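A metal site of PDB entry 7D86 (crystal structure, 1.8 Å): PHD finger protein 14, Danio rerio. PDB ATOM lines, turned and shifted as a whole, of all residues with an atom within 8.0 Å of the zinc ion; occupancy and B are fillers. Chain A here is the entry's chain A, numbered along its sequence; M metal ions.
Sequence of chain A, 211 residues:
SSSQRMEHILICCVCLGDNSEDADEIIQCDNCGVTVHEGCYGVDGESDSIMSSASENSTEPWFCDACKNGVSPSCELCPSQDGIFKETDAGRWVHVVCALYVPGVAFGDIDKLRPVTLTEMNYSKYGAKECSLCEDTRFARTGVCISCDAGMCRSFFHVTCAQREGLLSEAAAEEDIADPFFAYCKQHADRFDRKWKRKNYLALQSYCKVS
The zinc ion is bound by a ring nitrogen (ND1) of His 188 (2.1 Å). The zinc ion is bound by the side-chain sulfur (SG) of Cys 153 (2.3 Å). The side-chain sulfur (SG) of Cys 148 binds the zinc ion (2.3 Å). SG of Cys 185 binds the zinc ion (2.3 Å).
NH1 of Arg 154 lies within hydrogen-bond range of O of Cys 148 (3.4 Å). The backbone NH (N) of Cys 148 lies within hydrogen-bond range of the backbone carbonyl oxygen (O) of Ser 155 (2.9 Å). SG of Cys 153 lies close to OG of Ser 155 (3.6 Å). SG of Cys 185 lies close to N of Gln 187 (3.5 Å). The backbone carbonyl oxygen (O) of Cys 153 sits at hydrogen-bond distance from the side-chain hydroxyl (OG) of Ser 147 (3.2 Å). SG of Cys 148 lies close to N of Ala 150 (3.4 Å).
Of the 18 residues printed, 4 come within 4 Å of the zinc ion. Along chain A the residues within 4 Å of the zinc ion span positions 148 to 188.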
ATOM      1  N   SER A 147      -7.001  -5.046   4.577  1.00  0.00           N
ATOM      2  CA  SER A 147      -6.578  -5.357   3.228  1.00  0.00           C
ATOM      3  C   SER A 147      -6.828  -6.826   2.910  1.00  0.00           C
ATOM      4  O   SER A 147      -7.058  -7.649   3.809  1.00  0.00           O
ATOM      5  CB  SER A 147      -5.107  -5.054   3.004  1.00  0.00           C
ATOM      6  OG  SER A 147      -4.694  -5.522   1.737  1.00  0.00           O
ATOM      7  N   CYS A 148      -6.769  -7.138   1.625  1.00  0.00           N
ATOM      8  CA  CYS A 148      -6.870  -8.525   1.184  1.00  0.00           C
ATOM      9  C   CYS A 148      -5.698  -9.328   1.723  1.00  0.00           C
ATOM     10  O   CYS A 148      -4.571  -8.822   1.810  1.00  0.00           O
ATOM     11  CB  CYS A 148      -6.906  -8.585  -0.353  1.00  0.00           C
ATOM     12  SG  CYS A 148      -6.811 -10.259  -1.061  1.00  0.00           S
ATOM     13  N   ASP A 149      -5.965 -10.585   2.085  1.00  0.00           N
ATOM     14  CA  ASP A 149      -4.960 -11.426   2.719  1.00  0.00           C
ATOM     15  C   ASP A 149      -4.296 -12.409   1.759  1.00  0.00           C
ATOM     16  O   ASP A 149      -3.502 -13.239   2.202  1.00  0.00           O
ATOM     17  CB  ASP A 149      -5.573 -12.173   3.895  1.00  0.00           C
ATOM     18  CG  ASP A 149      -5.765 -11.277   5.112  1.00  0.00           C
ATOM     19  OD1 ASP A 149      -4.834 -10.516   5.433  1.00  0.00           O
ATOM     20  OD2 ASP A 149      -6.851 -11.307   5.703  1.00  0.00           O
ATOM     21  N   ALA A 150      -4.601 -12.340   0.467  1.00  0.00           N
ATOM     22  CA  ALA A 150      -3.995 -13.231  -0.510  1.00  0.00           C
ATOM     23  C   ALA A 150      -2.657 -12.668  -0.944  1.00  0.00           C
ATOM     24  O   ALA A 150      -2.536 -11.476  -1.234  1.00  0.00           O
ATOM     25  CB  ALA A 150      -4.917 -13.435  -1.707  1.00  0.00           C
ATOM     26  N   GLY A 151      -1.642 -13.532  -0.977  1.00  0.00           N
ATOM     27  CA  GLY A 151      -0.284 -13.145  -1.336  1.00  0.00           C
ATOM     28  C   GLY A 151       0.154 -11.828  -0.735  1.00  0.00           C
ATOM     29  O   GLY A 151       0.120 -11.632   0.484  1.00  0.00           O
ATOM     30  N   MET A 152       0.559 -10.902  -1.602  1.00  0.00           N
ATOM     31  CA  MET A 152       0.892  -9.534  -1.211  1.00  0.00           C
ATOM     32  C   MET A 152      -0.109  -8.533  -1.769  1.00  0.00           C
ATOM     33  O   MET A 152       0.240  -7.378  -2.059  1.00  0.00           O
ATOM     34  CB  MET A 152       2.317  -9.181  -1.656  1.00  0.00           C
ATOM     35  CG  MET A 152       3.394 -10.065  -1.042  1.00  0.00           C
ATOM     36  SD  MET A 152       3.609  -9.778   0.726  1.00  0.00           S
ATOM     37  CE  MET A 152       3.130 -11.360   1.398  1.00  0.00           C
ATOM     38  N   CYS A 153      -1.356  -8.965  -1.956  1.00  0.00           N
ATOM     39  CA  CYS A 153      -2.387  -8.101  -2.510  1.00  0.00           C
ATOM     40  C   CYS A 153      -2.645  -6.910  -1.600  1.00  0.00           C
ATOM     41  O   CYS A 153      -2.793  -7.049  -0.384  1.00  0.00           O
ATOM     42  CB  CYS A 153      -3.684  -8.880  -2.730  1.00  0.00           C
ATOM     43  SG  CYS A 153      -5.029  -7.913  -3.463  1.00  0.00           S
ATOM     44  N   ARG A 154      -2.724  -5.724  -2.207  1.00  0.00           N
ATOM     45  CA  ARG A 154      -3.007  -4.516  -1.447  1.00  0.00           C
ATOM     46  C   ARG A 154      -4.312  -3.877  -1.904  1.00  0.00           C
ATOM     47  O   ARG A 154      -4.306  -2.788  -2.481  1.00  0.00           O
ATOM     48  CB  ARG A 154      -1.838  -3.522  -1.569  1.00  0.00           C
ATOM     49  CG  ARG A 154      -0.536  -3.955  -0.890  1.00  0.00           C
ATOM     50  CD  ARG A 154      -0.637  -3.950   0.619  1.00  0.00           C
ATOM     51  NE  ARG A 154      -1.323  -5.142   1.131  1.00  0.00           N
ATOM     52  CZ  ARG A 154      -1.725  -5.302   2.381  1.00  0.00           C
ATOM     53  NH1 ARG A 154      -2.342  -6.421   2.734  1.00  0.00           N
ATOM     54  NH2 ARG A 154      -1.526  -4.341   3.275  1.00  0.00           N
ATOM     55  N   SER A 155      -5.425  -4.550  -1.660  1.00  0.00           N
ATOM     56  CA  SER A 155      -6.752  -3.983  -1.856  1.00  0.00           C
ATOM     57  C   SER A 155      -7.339  -3.662  -0.480  1.00  0.00           C
ATOM     58  O   SER A 155      -7.376  -4.538   0.385  1.00  0.00           O
ATOM     59  CB  SER A 155      -7.686  -4.955  -2.587  1.00  0.00           C
ATOM     60  OG  SER A 155      -7.266  -5.158  -3.929  1.00  0.00           O
ATOM     61  N   PHE A 156      -7.791  -2.429  -0.293  1.00  0.00           N
ATOM     62  CA  PHE A 156      -8.248  -1.968   1.016  1.00  0.00           C
ATOM     63  C   PHE A 156      -9.761  -1.748   1.050  1.00  0.00           C
ATOM     64  O   PHE A 156     -10.348  -1.271   0.073  1.00  0.00           O
ATOM     65  CB  PHE A 156      -7.538  -0.673   1.416  1.00  0.00           C
ATOM     66  CG  PHE A 156      -6.054  -0.812   1.523  1.00  0.00           C
ATOM     67  CD1 PHE A 156      -5.494  -1.546   2.558  1.00  0.00           C
ATOM     68  CD2 PHE A 156      -5.222  -0.242   0.586  1.00  0.00           C
ATOM     69  CE1 PHE A 156      -4.101  -1.698   2.648  1.00  0.00           C
ATOM     70  CE2 PHE A 156      -3.846  -0.393   0.674  1.00  0.00           C
ATOM     71  CZ  PHE A 156      -3.287  -1.126   1.709  1.00  0.00           C
ATOM     72  N   PHE A 157     -10.362  -2.064   2.197  1.00  0.00           N
ATOM     73  CA  PHE A 157     -11.790  -1.885   2.372  1.00  0.00           C
ATOM     74  C   PHE A 157     -12.134  -1.894   3.852  1.00  0.00           C
ATOM     75  O   PHE A 157     -11.422  -2.490   4.666  1.00  0.00           O
ATOM     76  CB  PHE A 157     -12.596  -2.978   1.644  1.00  0.00           C
ATOM     77  CG  PHE A 157     -11.866  -4.281   1.498  1.00  0.00           C
ATOM     78  CD1 PHE A 157     -11.614  -5.088   2.591  1.00  0.00           C
ATOM     79  CD2 PHE A 157     -11.442  -4.716   0.246  1.00  0.00           C
ATOM     80  CE1 PHE A 157     -10.930  -6.297   2.459  1.00  0.00           C
ATOM     81  CE2 PHE A 157     -10.772  -5.926   0.097  1.00  0.00           C
ATOM     82  CZ  PHE A 157     -10.523  -6.719   1.210  1.00  0.00           C
ATOM     83  N   ALA A 183      -9.547 -11.995   5.158  1.00  0.00           N
ATOM     84  CA  ALA A 183     -10.396 -11.418   4.125  1.00  0.00           C
ATOM     85  C   ALA A 183      -9.662 -11.400   2.794  1.00  0.00           C
ATOM     86  O   ALA A 183      -8.455 -11.145   2.742  1.00  0.00           O
ATOM     87  CB  ALA A 183     -10.826  -9.994   4.489  1.00  0.00           C
ATOM     88  N   TYR A 184     -10.407 -11.613   1.717  1.00  0.00           N
ATOM     89  CA  TYR A 184      -9.901 -11.590   0.351  1.00  0.00           C
ATOM     90  C   TYR A 184     -10.675 -10.581  -0.477  1.00  0.00           C
ATOM     91  O   TYR A 184     -11.900 -10.461  -0.340  1.00  0.00           O
ATOM     92  CB  TYR A 184     -10.017 -12.959  -0.325  1.00  0.00           C
ATOM     93  CG  TYR A 184      -9.150 -14.068   0.232  1.00  0.00           C
ATOM     94  CD1 TYR A 184      -7.862 -13.839   0.664  1.00  0.00           C
ATOM     95  CD2 TYR A 184      -9.652 -15.359   0.302  1.00  0.00           C
ATOM     96  CE1 TYR A 184      -7.077 -14.865   1.171  1.00  0.00           C
ATOM     97  CE2 TYR A 184      -8.890 -16.400   0.805  1.00  0.00           C
ATOM     98  CZ  TYR A 184      -7.601 -16.147   1.236  1.00  0.00           C
ATOM     99  OH  TYR A 184      -6.873 -17.187   1.734  1.00  0.00           O
ATOM    100  N   CYS A 185      -9.979  -9.868  -1.347  1.00  0.00           N
ATOM    101  CA  CYS A 185     -10.708  -9.002  -2.264  1.00  0.00           C
ATOM    102  C   CYS A 185     -11.531  -9.864  -3.228  1.00  0.00           C
ATOM    103  O   CYS A 185     -11.414 -11.097  -3.252  1.00  0.00           O
ATOM    104  CB  CYS A 185      -9.751  -8.109  -3.043  1.00  0.00           C
ATOM    105  SG  CYS A 185      -8.720  -9.023  -4.223  1.00  0.00           S
ATOM    106  N   LYS A 186     -12.364  -9.212  -4.040  1.00  0.00           N
ATOM    107  CA  LYS A 186     -13.219  -9.954  -4.961  1.00  0.00           C
ATOM    108  C   LYS A 186     -12.403 -10.787  -5.941  1.00  0.00           C
ATOM    109  O   LYS A 186     -12.834 -11.871  -6.341  1.00  0.00           O
ATOM    110  CB  LYS A 186     -14.134  -9.000  -5.738  1.00  0.00           C
ATOM    111  CG  LYS A 186     -15.153  -8.259  -4.883  1.00  0.00           C
ATOM    112  CD  LYS A 186     -16.016  -7.376  -5.768  1.00  0.00           C
ATOM    113  CE  LYS A 186     -16.882  -6.435  -4.935  1.00  0.00           C
ATOM    114  NZ  LYS A 186     -17.714  -5.540  -5.794  1.00  0.00           N
ATOM    115  N   GLN A 187     -11.232 -10.299  -6.348  1.00  0.00           N
ATOM    116  CA  GLN A 187     -10.457 -11.046  -7.312  1.00  0.00           C
ATOM    117  C   GLN A 187      -9.905 -12.345  -6.719  1.00  0.00           C
ATOM    118  O   GLN A 187      -9.729 -13.327  -7.451  1.00  0.00           O
ATOM    119  CB  GLN A 187      -9.310 -10.193  -7.860  1.00  0.00           C
ATOM    120  CG  GLN A 187      -8.626 -10.804  -9.066  1.00  0.00           C
ATOM    121  CD  GLN A 187      -7.478  -9.944  -9.578  1.00  0.00           C
ATOM    122  OE1 GLN A 187      -7.070  -8.982  -8.927  1.00  0.00           O
ATOM    123  NE2 GLN A 187      -6.961 -10.293 -10.741  1.00  0.00           N
ATOM    124  N   HIS A 188      -9.684 -12.379  -5.409  1.00  0.00           N
ATOM    125  CA  HIS A 188      -9.001 -13.506  -4.783  1.00  0.00           C
ATOM    126  C   HIS A 188      -9.909 -14.351  -3.905  1.00  0.00           C
ATOM    127  O   HIS A 188      -9.427 -15.321  -3.299  1.00  0.00           O
ATOM    128  CB  HIS A 188      -7.817 -12.985  -3.974  1.00  0.00           C
ATOM    129  CG  HIS A 188      -6.759 -12.339  -4.817  1.00  0.00           C
ATOM    130  ND1 HIS A 188      -6.192 -11.118  -4.524  1.00  0.00           N
ATOM    131  CD2 HIS A 188      -6.164 -12.757  -5.975  1.00  0.00           C
ATOM    132  CE1 HIS A 188      -5.305 -10.807  -5.438  1.00  0.00           C
ATOM    133  NE2 HIS A 188      -5.263 -11.785  -6.338  1.00  0.00           N
ATOM    134  N   ALA A 189     -11.194 -14.025  -3.809  1.00  0.00           N
ATOM    135  CA  ALA A 189     -12.076 -14.699  -2.874  1.00  0.00           C
ATOM    136  C   ALA A 189     -12.535 -16.052  -3.404  1.00  0.00           C
ATOM    137  O   ALA A 189     -12.547 -16.310  -4.612  1.00  0.00           O
ATOM    138  CB  ALA A 189     -13.308 -13.840  -2.592  1.00  0.00           C
HETATM  139 ZN    ZN M   1      -6.650  -9.545  -3.268  1.00  0.00          ZN
